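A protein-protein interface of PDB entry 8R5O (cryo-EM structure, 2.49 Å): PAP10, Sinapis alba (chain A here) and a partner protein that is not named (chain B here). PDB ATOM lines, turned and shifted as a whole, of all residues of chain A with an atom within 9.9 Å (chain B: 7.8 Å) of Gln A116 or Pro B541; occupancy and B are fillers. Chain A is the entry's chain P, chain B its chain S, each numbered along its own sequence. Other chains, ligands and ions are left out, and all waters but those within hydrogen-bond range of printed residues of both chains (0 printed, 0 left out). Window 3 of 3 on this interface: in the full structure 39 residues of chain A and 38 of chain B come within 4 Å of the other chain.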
ATOM      1  N   VAL A  79     -13.089  -0.598 -12.591  1.00  0.00           N
ATOM      2  CA  VAL A  79     -13.714  -1.903 -12.412  1.00  0.00           C
ATOM      3  C   VAL A  79     -14.583  -2.184 -13.631  1.00  0.00           C
ATOM      4  O   VAL A  79     -15.465  -1.389 -13.973  1.00  0.00           O
ATOM      5  CB  VAL A  79     -14.538  -1.950 -11.118  1.00  0.00           C
ATOM      6  CG1 VAL A  79     -15.122  -3.337 -10.905  1.00  0.00           C
ATOM      7  CG2 VAL A  79     -13.679  -1.540  -9.930  1.00  0.00           C
ATOM      8  N   ASP A 102     -15.659  -9.827  -8.474  1.00  0.00           N
ATOM      9  CA  ASP A 102     -16.728  -9.361  -7.595  1.00  0.00           C
ATOM     10  C   ASP A 102     -18.061  -9.868  -8.137  1.00  0.00           C
ATOM     11  O   ASP A 102     -18.653  -9.254  -9.029  1.00  0.00           O
ATOM     12  CB  ASP A 102     -16.703  -7.839  -7.490  1.00  0.00           C
ATOM     13  CG  ASP A 102     -17.956  -7.272  -6.851  1.00  0.00           C
ATOM     14  OD1 ASP A 102     -18.238  -7.606  -5.681  1.00  0.00           O
ATOM     15  OD2 ASP A 102     -18.657  -6.483  -7.519  1.00  0.00           O
ATOM     16  N   GLY A 109     -28.514  -4.658  -1.927  1.00  0.00           N
ATOM     17  CA  GLY A 109     -28.049  -3.431  -1.327  1.00  0.00           C
ATOM     18  C   GLY A 109     -26.596  -3.447  -0.886  1.00  0.00           C
ATOM     19  O   GLY A 109     -25.835  -2.526  -1.194  1.00  0.00           O
ATOM     20  N   PRO A 110     -26.178  -4.480  -0.141  1.00  0.00           N
ATOM     21  CA  PRO A 110     -24.764  -4.550   0.265  1.00  0.00           C
ATOM     22  C   PRO A 110     -23.789  -4.636  -0.897  1.00  0.00           C
ATOM     23  O   PRO A 110     -22.637  -4.213  -0.753  1.00  0.00           O
ATOM     24  CB  PRO A 110     -24.715  -5.810   1.139  1.00  0.00           C
ATOM     25  CG  PRO A 110     -26.086  -5.925   1.688  1.00  0.00           C
ATOM     26  CD  PRO A 110     -27.004  -5.452   0.599  1.00  0.00           C
ATOM     27  N   CYS A 111     -24.205  -5.182  -2.042  1.00  0.00           N
ATOM     28  CA  CYS A 111     -23.323  -5.206  -3.206  1.00  0.00           C
ATOM     29  C   CYS A 111     -23.015  -3.800  -3.701  1.00  0.00           C
ATOM     30  O   CYS A 111     -21.941  -3.561  -4.261  1.00  0.00           O
ATOM     31  CB  CYS A 111     -23.943  -6.039  -4.327  1.00  0.00           C
ATOM     32  SG  CYS A 111     -23.913  -7.819  -4.040  1.00  0.00           S
ATOM     33  N   ILE A 112     -23.943  -2.860  -3.506  1.00  0.00           N
ATOM     34  CA  ILE A 112     -23.694  -1.473  -3.876  1.00  0.00           C
ATOM     35  C   ILE A 112     -22.659  -0.852  -2.948  1.00  0.00           C
ATOM     36  O   ILE A 112     -21.784  -0.096  -3.387  1.00  0.00           O
ATOM     37  CB  ILE A 112     -25.016  -0.684  -3.876  1.00  0.00           C
ATOM     38  CG1 ILE A 112     -26.074  -1.439  -4.682  1.00  0.00           C
ATOM     39  CG2 ILE A 112     -24.811   0.713  -4.432  1.00  0.00           C
ATOM     40  CD1 ILE A 112     -27.338  -0.654  -4.940  1.00  0.00           C
ATOM     41  N   LEU A 113     -22.740  -1.159  -1.649  1.00  0.00           N
ATOM     42  CA  LEU A 113     -21.716  -0.711  -0.707  1.00  0.00           C
ATOM     43  C   LEU A 113     -20.363  -1.332  -1.027  1.00  0.00           C
ATOM     44  O   LEU A 113     -19.325  -0.674  -0.897  1.00  0.00           O
ATOM     45  CB  LEU A 113     -22.129  -1.051   0.724  1.00  0.00           C
ATOM     46  CG  LEU A 113     -23.262  -0.247   1.353  1.00  0.00           C
ATOM     47  CD1 LEU A 113     -23.724  -0.910   2.639  1.00  0.00           C
ATOM     48  CD2 LEU A 113     -22.814   1.177   1.618  1.00  0.00           C
ATOM     49  N   MET A 114     -20.356  -2.605  -1.427  1.00  0.00           N
ATOM     50  CA  MET A 114     -19.111  -3.261  -1.811  1.00  0.00           C
ATOM     51  C   MET A 114     -18.491  -2.602  -3.037  1.00  0.00           C
ATOM     52  O   MET A 114     -17.262  -2.548  -3.159  1.00  0.00           O
ATOM     53  CB  MET A 114     -19.367  -4.748  -2.067  1.00  0.00           C
ATOM     54  CG  MET A 114     -18.180  -5.520  -2.623  1.00  0.00           C
ATOM     55  SD  MET A 114     -16.791  -5.643  -1.481  1.00  0.00           S
ATOM     56  CE  MET A 114     -17.450  -6.762  -0.245  1.00  0.00           C
ATOM     57  N   ALA A 115     -19.322  -2.095  -3.949  1.00  0.00           N
ATOM     58  CA  ALA A 115     -18.806  -1.404  -5.125  1.00  0.00           C
ATOM     59  C   ALA A 115     -18.023  -0.158  -4.734  1.00  0.00           C
ATOM     60  O   ALA A 115     -16.997   0.158  -5.350  1.00  0.00           O
ATOM     61  CB  ALA A 115     -19.956  -1.048  -6.066  1.00  0.00           C
ATOM     62  N   GLN A 116     -18.489   0.566  -3.713  1.00  0.00           N
ATOM     63  CA  GLN A 116     -17.776   1.756  -3.256  1.00  0.00           C
ATOM     64  C   GLN A 116     -16.416   1.404  -2.663  1.00  0.00           C
ATOM     65  O   GLN A 116     -15.436   2.122  -2.884  1.00  0.00           O
ATOM     66  CB  GLN A 116     -18.619   2.516  -2.234  1.00  0.00           C
ATOM     67  CG  GLN A 116     -19.872   3.147  -2.801  1.00  0.00           C
ATOM     68  CD  GLN A 116     -20.640   3.940  -1.764  1.00  0.00           C
ATOM     69  OE1 GLN A 116     -20.397   3.812  -0.565  1.00  0.00           O
ATOM     70  NE2 GLN A 116     -21.571   4.765  -2.221  1.00  0.00           N
ATOM     71  N   GLU A 117     -16.341   0.318  -1.888  1.00  0.00           N
ATOM     72  CA  GLU A 117     -15.055  -0.103  -1.338  1.00  0.00           C
ATOM     73  C   GLU A 117     -14.090  -0.519  -2.441  1.00  0.00           C
ATOM     74  O   GLU A 117     -12.900  -0.195  -2.388  1.00  0.00           O
ATOM     75  CB  GLU A 117     -15.247  -1.252  -0.349  1.00  0.00           C
ATOM     76  CG  GLU A 117     -15.879  -0.851   0.970  1.00  0.00           C
ATOM     77  CD  GLU A 117     -15.966  -2.003   1.950  1.00  0.00           C
ATOM     78  OE1 GLU A 117     -16.282  -3.131   1.523  1.00  0.00           O
ATOM     79  OE2 GLU A 117     -15.711  -1.782   3.151  1.00  0.00           O
ATOM     80  N   LEU A 118     -14.586  -1.240  -3.449  1.00  0.00           N
ATOM     81  CA  LEU A 118     -13.703  -1.783  -4.474  1.00  0.00           C
ATOM     82  C   LEU A 118     -13.122  -0.695  -5.369  1.00  0.00           C
ATOM     83  O   LEU A 118     -11.990  -0.833  -5.846  1.00  0.00           O
ATOM     84  CB  LEU A 118     -14.445  -2.819  -5.313  1.00  0.00           C
ATOM     85  CG  LEU A 118     -14.789  -4.116  -4.579  1.00  0.00           C
ATOM     86  CD1 LEU A 118     -15.500  -5.081  -5.507  1.00  0.00           C
ATOM     87  CD2 LEU A 118     -13.537  -4.747  -3.996  1.00  0.00           C
ATOM     88  N   GLU A 119     -13.869   0.380  -5.618  1.00  0.00           N
ATOM     89  CA  GLU A 119     -13.324   1.450  -6.445  1.00  0.00           C
ATOM     90  C   GLU A 119     -12.292   2.273  -5.688  1.00  0.00           C
ATOM     91  O   GLU A 119     -11.363   2.805  -6.302  1.00  0.00           O
ATOM     92  CB  GLU A 119     -14.446   2.341  -6.981  1.00  0.00           C
ATOM     93  CG  GLU A 119     -15.301   3.008  -5.923  1.00  0.00           C
ATOM     94  CD  GLU A 119     -16.472   3.762  -6.518  1.00  0.00           C
ATOM     95  OE1 GLU A 119     -16.507   3.932  -7.756  1.00  0.00           O
ATOM     96  OE2 GLU A 119     -17.365   4.183  -5.752  1.00  0.00           O
ATOM     97  N   MET A 120     -12.434   2.389  -4.366  1.00  0.00           N
ATOM     98  CA  MET A 120     -11.356   2.959  -3.565  1.00  0.00           C
ATOM     99  C   MET A 120     -10.119   2.070  -3.608  1.00  0.00           C
ATOM    100  O   MET A 120      -8.993   2.565  -3.739  1.00  0.00           O
ATOM    101  CB  MET A 120     -11.819   3.170  -2.123  1.00  0.00           C
ATOM    102  CG  MET A 120     -10.668   3.353  -1.152  1.00  0.00           C
ATOM    103  SD  MET A 120     -11.085   4.295   0.322  1.00  0.00           S
ATOM    104  CE  MET A 120     -11.509   5.876  -0.400  1.00  0.00           C
ATOM    105  N   LEU A 121     -10.309   0.753  -3.497  1.00  0.00           N
ATOM    106  CA  LEU A 121      -9.186  -0.174  -3.565  1.00  0.00           C
ATOM    107  C   LEU A 121      -8.513  -0.128  -4.931  1.00  0.00           C
ATOM    108  O   LEU A 121      -7.282  -0.187  -5.024  1.00  0.00           O
ATOM    109  CB  LEU A 121      -9.660  -1.593  -3.246  1.00  0.00           C
ATOM    110  CG  LEU A 121      -8.607  -2.698  -3.175  1.00  0.00           C
ATOM    111  CD1 LEU A 121      -7.756  -2.556  -1.926  1.00  0.00           C
ATOM    112  CD2 LEU A 121      -9.268  -4.065  -3.228  1.00  0.00           C
ATOM    113  N   ALA A 122      -9.306  -0.028  -6.000  1.00  0.00           N
ATOM    114  CA  ALA A 122      -8.739   0.035  -7.344  1.00  0.00           C
ATOM    115  C   ALA A 122      -7.865   1.270  -7.516  1.00  0.00           C
ATOM    116  O   ALA A 122      -6.845   1.225  -8.213  1.00  0.00           O
ATOM    117  CB  ALA A 122      -9.857   0.018  -8.383  1.00  0.00           C
ATOM    118  N   VAL A 123      -8.251   2.384  -6.894  1.00  0.00           N
ATOM    119  CA  VAL A 123      -7.448   3.599  -6.981  1.00  0.00           C
ATOM    120  C   VAL A 123      -6.150   3.444  -6.201  1.00  0.00           C
ATOM    121  O   VAL A 123      -5.089   3.908  -6.637  1.00  0.00           O
ATOM    122  CB  VAL A 123      -8.265   4.812  -6.497  1.00  0.00           C
ATOM    123  CG1 VAL A 123      -7.379   6.038  -6.370  1.00  0.00           C
ATOM    124  CG2 VAL A 123      -9.413   5.087  -7.454  1.00  0.00           C
ATOM    125  N   GLU A 124      -6.205   2.796  -5.034  1.00  0.00           N
ATOM    126  CA  GLU A 124      -4.992   2.574  -4.252  1.00  0.00           C
ATOM    127  C   GLU A 124      -3.990   1.729  -5.029  1.00  0.00           C
ATOM    128  O   GLU A 124      -2.815   2.091  -5.152  1.00  0.00           O
ATOM    129  CB  GLU A 124      -5.340   1.907  -2.921  1.00  0.00           C
ATOM    130  CG  GLU A 124      -4.134   1.590  -2.049  1.00  0.00           C
ATOM    131  CD  GLU A 124      -4.488   0.731  -0.851  1.00  0.00           C
ATOM    132  OE1 GLU A 124      -5.654   0.295  -0.758  1.00  0.00           O
ATOM    133  OE2 GLU A 124      -3.602   0.491  -0.005  1.00  0.00           O
ATOM    134  N   ILE A 131      -9.493  -5.496 -10.836  1.00  0.00           N
ATOM    135  CA  ILE A 131     -10.786  -5.746 -10.211  1.00  0.00           C
ATOM    136  C   ILE A 131     -11.828  -5.851 -11.312  1.00  0.00           C
ATOM    137  O   ILE A 131     -11.997  -4.918 -12.106  1.00  0.00           O
ATOM    138  CB  ILE A 131     -11.161  -4.647  -9.205  1.00  0.00           C
ATOM    139  CG1 ILE A 131     -10.163  -4.623  -8.048  1.00  0.00           C
ATOM    140  CG2 ILE A 131     -12.575  -4.857  -8.688  1.00  0.00           C
ATOM    141  CD1 ILE A 131     -10.423  -3.527  -7.046  1.00  0.00           C
ATOM    142  N   LYS A 133     -15.983  -7.496 -12.194  1.00  0.00           N
ATOM    143  CA  LYS A 133     -17.241  -7.905 -11.593  1.00  0.00           C
ATOM    144  C   LYS A 133     -18.059  -8.711 -12.589  1.00  0.00           C
ATOM    145  O   LYS A 133     -18.027  -8.461 -13.797  1.00  0.00           O
ATOM    146  CB  LYS A 133     -18.050  -6.700 -11.090  1.00  0.00           C
ATOM    147  CG  LYS A 133     -18.386  -5.665 -12.143  1.00  0.00           C
ATOM    148  CD  LYS A 133     -19.180  -4.524 -11.528  1.00  0.00           C
ATOM    149  CE  LYS A 133     -19.563  -3.481 -12.560  1.00  0.00           C
ATOM    150  NZ  LYS A 133     -18.387  -2.701 -13.032  1.00  0.00           N
ATOM    151  N   PRO A 152     -22.652 -10.149  -1.014  1.00  0.00           N
ATOM    152  CA  PRO A 152     -21.554 -10.072  -1.989  1.00  0.00           C
ATOM    153  C   PRO A 152     -20.519 -11.180  -1.804  1.00  0.00           C
ATOM    154  O   PRO A 152     -20.388 -11.752  -0.724  1.00  0.00           O
ATOM    155  CB  PRO A 152     -20.964  -8.682  -1.721  1.00  0.00           C
ATOM    156  CG  PRO A 152     -21.187  -8.471  -0.255  1.00  0.00           C
ATOM    157  CD  PRO A 152     -22.513  -9.130   0.044  1.00  0.00           C
ATOM    158  N   LEU A 154     -16.377 -12.159  -3.112  1.00  0.00           N
ATOM    159  CA  LEU A 154     -15.158 -11.773  -3.805  1.00  0.00           C
ATOM    160  C   LEU A 154     -14.255 -12.983  -3.979  1.00  0.00           C
ATOM    161  O   LEU A 154     -14.150 -13.826  -3.084  1.00  0.00           O
ATOM    162  CB  LEU A 154     -14.405 -10.676  -3.048  1.00  0.00           C
ATOM    163  CG  LEU A 154     -15.186  -9.424  -2.650  1.00  0.00           C
ATOM    164  CD1 LEU A 154     -14.270  -8.435  -1.958  1.00  0.00           C
ATOM    165  CD2 LEU A 154     -15.847  -8.792  -3.860  1.00  0.00           C
ATOM    166  N   LEU A 171     -19.760  -8.265   3.559  1.00  0.00           N
ATOM    167  CA  LEU A 171     -19.148  -6.946   3.428  1.00  0.00           C
ATOM    168  C   LEU A 171     -17.943  -6.893   4.360  1.00  0.00           C
ATOM    169  O   LEU A 171     -18.083  -6.664   5.564  1.00  0.00           O
ATOM    170  CB  LEU A 171     -20.165  -5.855   3.744  1.00  0.00           C
ATOM    171  CG  LEU A 171     -19.917  -4.440   3.229  1.00  0.00           C
ATOM    172  CD1 LEU A 171     -19.533  -4.455   1.760  1.00  0.00           C
ATOM    173  CD2 LEU A 171     -21.168  -3.608   3.439  1.00  0.00           C
ATOM    174  N   ILE A 172     -16.755  -7.104   3.804  1.00  0.00           N
ATOM    175  CA  ILE A 172     -15.527  -7.152   4.594  1.00  0.00           C
ATOM    176  C   ILE A 172     -14.841  -5.792   4.543  1.00  0.00           C
ATOM    177  O   ILE A 172     -14.955  -5.078   3.539  1.00  0.00           O
ATOM    178  CB  ILE A 172     -14.591  -8.267   4.099  1.00  0.00           C
ATOM    179  CG1 ILE A 172     -14.313  -8.114   2.602  1.00  0.00           C
ATOM    180  CG2 ILE A 172     -15.181  -9.634   4.413  1.00  0.00           C
ATOM    181  CD1 ILE A 172     -13.284  -9.084   2.061  1.00  0.00           C
ATOM    182  N   LEU A 174     -11.940  -2.796   4.253  1.00  0.00           N
ATOM    183  CA  LEU A 174     -10.899  -2.577   3.254  1.00  0.00           C
ATOM    184  C   LEU A 174      -9.572  -3.190   3.680  1.00  0.00           C
ATOM    185  O   LEU A 174      -8.842  -3.741   2.850  1.00  0.00           O
ATOM    186  CB  LEU A 174     -10.724  -1.082   3.000  1.00  0.00           C
ATOM    187  CG  LEU A 174     -10.959  -0.554   1.587  1.00  0.00           C
ATOM    188  CD1 LEU A 174     -10.573   0.909   1.526  1.00  0.00           C
ATOM    189  CD2 LEU A 174     -10.183  -1.359   0.558  1.00  0.00           C
ATOM    190  N   MET A 177      -8.973  -6.748   2.628  1.00  0.00           N
ATOM    191  CA  MET A 177      -8.607  -6.884   1.222  1.00  0.00           C
ATOM    192  C   MET A 177      -7.134  -6.564   1.003  1.00  0.00           C
ATOM    193  O   MET A 177      -6.449  -7.252   0.239  1.00  0.00           O
ATOM    194  CB  MET A 177      -9.478  -5.977   0.354  1.00  0.00           C
ATOM    195  CG  MET A 177     -10.966  -6.227   0.470  1.00  0.00           C
ATOM    196  SD  MET A 177     -11.900  -5.125  -0.606  1.00  0.00           S
ATOM    197  CE  MET A 177     -13.555  -5.380   0.010  1.00  0.00           C
ATOM    198  N   PHE B 483     -29.183   0.937  -0.706  1.00  0.00           N
ATOM    199  CA  PHE B 483     -28.420   0.128   0.235  1.00  0.00           C
ATOM    200  C   PHE B 483     -29.273  -0.884   0.997  1.00  0.00           C
ATOM    201  O   PHE B 483     -28.710  -1.776   1.639  1.00  0.00           O
ATOM    202  CB  PHE B 483     -27.696   1.032   1.238  1.00  0.00           C
ATOM    203  CG  PHE B 483     -26.616   1.883   0.629  1.00  0.00           C
ATOM    204  CD1 PHE B 483     -25.878   1.431  -0.452  1.00  0.00           C
ATOM    205  CD2 PHE B 483     -26.336   3.137   1.147  1.00  0.00           C
ATOM    206  CE1 PHE B 483     -24.885   2.217  -1.006  1.00  0.00           C
ATOM    207  CE2 PHE B 483     -25.344   3.923   0.600  1.00  0.00           C
ATOM    208  CZ  PHE B 483     -24.615   3.462  -0.479  1.00  0.00           C
ATOM    209  N   GLY B 538     -28.774   5.084   4.834  1.00  0.00           N
ATOM    210  CA  GLY B 538     -28.893   6.230   3.957  1.00  0.00           C
ATOM    211  C   GLY B 538     -28.852   5.853   2.481  1.00  0.00           C
ATOM    212  O   GLY B 538     -29.144   4.725   2.082  1.00  0.00           O
ATOM    213  N   TYR B 539     -28.467   6.835   1.666  1.00  0.00           N
ATOM    214  CA  TYR B 539     -28.478   6.747   0.214  1.00  0.00           C
ATOM    215  C   TYR B 539     -27.076   6.925  -0.354  1.00  0.00           C
ATOM    216  O   TYR B 539     -26.258   7.650   0.217  1.00  0.00           O
ATOM    217  CB  TYR B 539     -29.387   7.818  -0.403  1.00  0.00           C
ATOM    218  CG  TYR B 539     -30.860   7.662  -0.119  1.00  0.00           C
ATOM    219  CD1 TYR B 539     -31.399   8.056   1.098  1.00  0.00           C
ATOM    220  CD2 TYR B 539     -31.719   7.146  -1.079  1.00  0.00           C
ATOM    221  CE1 TYR B 539     -32.748   7.924   1.356  1.00  0.00           C
ATOM    222  CE2 TYR B 539     -33.070   7.014  -0.829  1.00  0.00           C
ATOM    223  CZ  TYR B 539     -33.578   7.404   0.389  1.00  0.00           C
ATOM    224  OH  TYR B 539     -34.921   7.270   0.641  1.00  0.00           O
ATOM    225  N   PRO B 540     -26.772   6.285  -1.486  1.00  0.00           N
ATOM    226  CA  PRO B 540     -25.534   6.608  -2.190  1.00  0.00           C
ATOM    227  C   PRO B 540     -25.599   8.008  -2.766  1.00  0.00           C
ATOM    228  O   PRO B 540     -26.684   8.502  -3.118  1.00  0.00           O
ATOM    229  CB  PRO B 540     -25.471   5.544  -3.302  1.00  0.00           C
ATOM    230  CG  PRO B 540     -26.880   5.141  -3.510  1.00  0.00           C
ATOM    231  CD  PRO B 540     -27.531   5.219  -2.159  1.00  0.00           C
ATOM    232  N   PRO B 541     -24.455   8.698  -2.887  1.00  0.00           N
ATOM    233  CA  PRO B 541     -24.430  10.076  -3.386  1.00  0.00           C
ATOM    234  C   PRO B 541     -24.638  10.161  -4.893  1.00  0.00           C
ATOM    235  O   PRO B 541     -25.781  10.108  -5.347  1.00  0.00           O
ATOM    236  CB  PRO B 541     -23.032  10.553  -3.002  1.00  0.00           C
ATOM    237  CG  PRO B 541     -22.210   9.319  -3.035  1.00  0.00           C
ATOM    238  CD  PRO B 541     -23.104   8.205  -2.569  1.00  0.00           C
ATOM    239  N   ASN B 562     -12.124   1.856   4.342  1.00  0.00           N
ATOM    240  CA  ASN B 562     -13.409   1.493   3.756  1.00  0.00           C
ATOM    241  C   ASN B 562     -14.116   2.726   3.224  1.00  0.00           C
ATOM    242  O   ASN B 562     -14.957   3.303   3.916  1.00  0.00           O
ATOM    243  CB  ASN B 562     -14.302   0.797   4.786  1.00  0.00           C
ATOM    244  CG  ASN B 562     -13.512   0.093   5.865  1.00  0.00           C
ATOM    245  OD1 ASN B 562     -12.535  -0.599   5.589  1.00  0.00           O
ATOM    246  ND2 ASN B 562     -13.932   0.271   7.110  1.00  0.00           N
ATOM    247  N   GLY B 563     -13.781   3.139   2.007  1.00  0.00           N
ATOM    248  CA  GLY B 563     -14.439   4.303   1.451  1.00  0.00           C
ATOM    249  C   GLY B 563     -15.889   4.018   1.134  1.00  0.00           C
ATOM    250  O   GLY B 563     -16.204   3.362   0.137  1.00  0.00           O
ATOM    251  N   ILE B 564     -16.783   4.526   1.975  1.00  0.00           N
ATOM    252  CA  ILE B 564     -18.220   4.352   1.814  1.00  0.00           C
ATOM    253  C   ILE B 564     -18.870   5.718   1.957  1.00  0.00           C
ATOM    254  O   ILE B 564     -18.660   6.410   2.959  1.00  0.00           O
ATOM    255  CB  ILE B 564     -18.788   3.345   2.829  1.00  0.00           C
ATOM    256  CG1 ILE B 564     -18.458   1.920   2.377  1.00  0.00           C
ATOM    257  CG2 ILE B 564     -20.289   3.523   2.979  1.00  0.00           C
ATOM    258  CD1 ILE B 564     -18.111   0.980   3.494  1.00  0.00           C
ATOM    259  N   ARG B 565     -19.649   6.105   0.953  1.00  0.00           N
ATOM    260  CA  ARG B 565     -20.213   7.442   0.858  1.00  0.00           C
ATOM    261  C   ARG B 565     -21.728   7.336   0.929  1.00  0.00           C
ATOM    262  O   ARG B 565     -22.342   6.642   0.111  1.00  0.00           O
ATOM    263  CB  ARG B 565     -19.772   8.123  -0.440  1.00  0.00           C
ATOM    264  CG  ARG B 565     -18.298   7.927  -0.764  1.00  0.00           C
ATOM    265  CD  ARG B 565     -17.915   8.578  -2.082  1.00  0.00           C
ATOM    266  NE  ARG B 565     -18.702   8.069  -3.199  1.00  0.00           N
ATOM    267  CZ  ARG B 565     -18.396   6.990  -3.906  1.00  0.00           C
ATOM    268  NH1 ARG B 565     -17.325   6.263  -3.629  1.00  0.00           N
ATOM    269  NH2 ARG B 565     -19.182   6.631  -4.917  1.00  0.00           N
ATOM    270  N   SER B 566     -22.325   8.014   1.903  1.00  0.00           N
ATOM    271  CA  SER B 566     -23.767   7.993   2.074  1.00  0.00           C
ATOM    272  C   SER B 566     -24.262   9.392   2.406  1.00  0.00           C
ATOM    273  O   SER B 566     -23.541  10.203   2.989  1.00  0.00           O
ATOM    274  CB  SER B 566     -24.200   7.010   3.172  1.00  0.00           C
ATOM    275  OG  SER B 566     -23.821   7.471   4.455  1.00  0.00           O
ATOM    276  N   ILE B 567     -25.510   9.659   2.026  1.00  0.00           N
ATOM    277  CA  ILE B 567     -26.181  10.915   2.316  1.00  0.00           C
ATOM    278  C   ILE B 567     -27.514  10.593   2.974  1.00  0.00           C
ATOM    279  O   ILE B 567     -28.046   9.488   2.842  1.00  0.00           O
ATOM    280  CB  ILE B 567     -26.397  11.774   1.051  1.00  0.00           C
ATOM    281  CG1 ILE B 567     -27.328  11.053   0.078  1.00  0.00           C
ATOM    282  CG2 ILE B 567     -25.070  12.096   0.384  1.00  0.00           C
ATOM    283  CD1 ILE B 567     -27.660  11.848  -1.158  1.00  0.00           C
ATOM    284  N   TYR B 572     -31.034  13.549  -0.116  1.00  0.00           N
ATOM    285  CA  TYR B 572     -31.489  12.867  -1.320  1.00  0.00           C
ATOM    286  C   TYR B 572     -32.665  13.588  -1.966  1.00  0.00           C
ATOM    287  O   TYR B 572     -32.814  13.552  -3.192  1.00  0.00           O
ATOM    288  CB  TYR B 572     -31.865  11.421  -0.995  1.00  0.00           C
ATOM    289  CG  TYR B 572     -32.454  10.655  -2.155  1.00  0.00           C
ATOM    290  CD1 TYR B 572     -31.641  10.103  -3.136  1.00  0.00           C
ATOM    291  CD2 TYR B 572     -33.825  10.477  -2.268  1.00  0.00           C
ATOM    292  CE1 TYR B 572     -32.181   9.399  -4.196  1.00  0.00           C
ATOM    293  CE2 TYR B 572     -34.369   9.777  -3.322  1.00  0.00           C
ATOM    294  CZ  TYR B 572     -33.546   9.241  -4.282  1.00  0.00           C
ATOM    295  OH  TYR B 572     -34.101   8.544  -5.329  1.00  0.00           O
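Of the printed residues of chain B, Gln A116 touches Phe B483, Pro B541, Gly B563, Ile B564 and Arg B565. No residue of chain B comes within 4 Å of Ala A115. No residue of chain A comes within 4 Å of Pro B540. Arg B565 touches two residues of chain A. Of the printed residues of chain A, Phe B483 touches Gly A109 (3.5 Å), Ile A112 (3.7 Å), Leu A113 (3.5 Å) and Gln A116 (3.7 Å). Of the printed residues of chain B, Ile A112 touches Phe B483 (3.7 Å). Printed residues of chain B within 4 Å of Glu A117: Asn B562 (3.4 Å), Gly B563 (3.7 Å) and Ile B564 (3.7 Å). Of the printed residues of chain B, Leu A113 touches Phe B483 and Ile B564. Glu A124 touches none of the printed residues of chain B. Ile A131 touches none of the printed residues of chain B.
Among the printed residues, pairs that only touch across the chains: Gln A116 with Ile B564 (3.3 Å), Glu A117 with Asn B562 (3.4 Å), Gly A109 with Phe B483 (3.5 Å), Leu A113 with Phe B483 (3.5 Å), Glu A117 with Gly B563 (3.7 Å), Glu A117 with Ile B564 (3.7 Å), Leu A113 with Ile B564 (3.7 Å), Gln A116 with Phe B483 (3.7 Å), Ile A112 with Phe B483 (3.7 Å), Gln A116 with Pro B541 (3.8 Å) and Leu A174 with Gly B563 (3.9 Å).
The side-chain amide oxygen of Gln A116 sits at hydrogen-bond distance from the backbone NH of Arg B565 (2.8 Å). The guanidinium group of Arg B565 is in salt-bridge range of the side-chain carboxylate of Glu A119 (3.0 Å). SD of Met A120 lies within hydrogen-bond range of N of Gly B563 (3.4 Å). The backbone NH (N) of Leu A174 lies within hydrogen-bond range of the side-chain amide oxygen (OD1) of Asn B562, 2.6 Å away. The backbone carbonyl oxygen of Gly B563 sits close to the backbone carbonyl oxygen of Gln A116.
Along chain B the printed residues that touch a printed residue of chain A span positions 483 to 565. Of the 26 printed residues of chain A, 8 touch a printed residue of chain B. Among the printed residues, Asp or Glu carboxylates within 4 Å of a Lys or Arg side-chain nitrogen of the other chain: Glu A119 with Arg B565.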
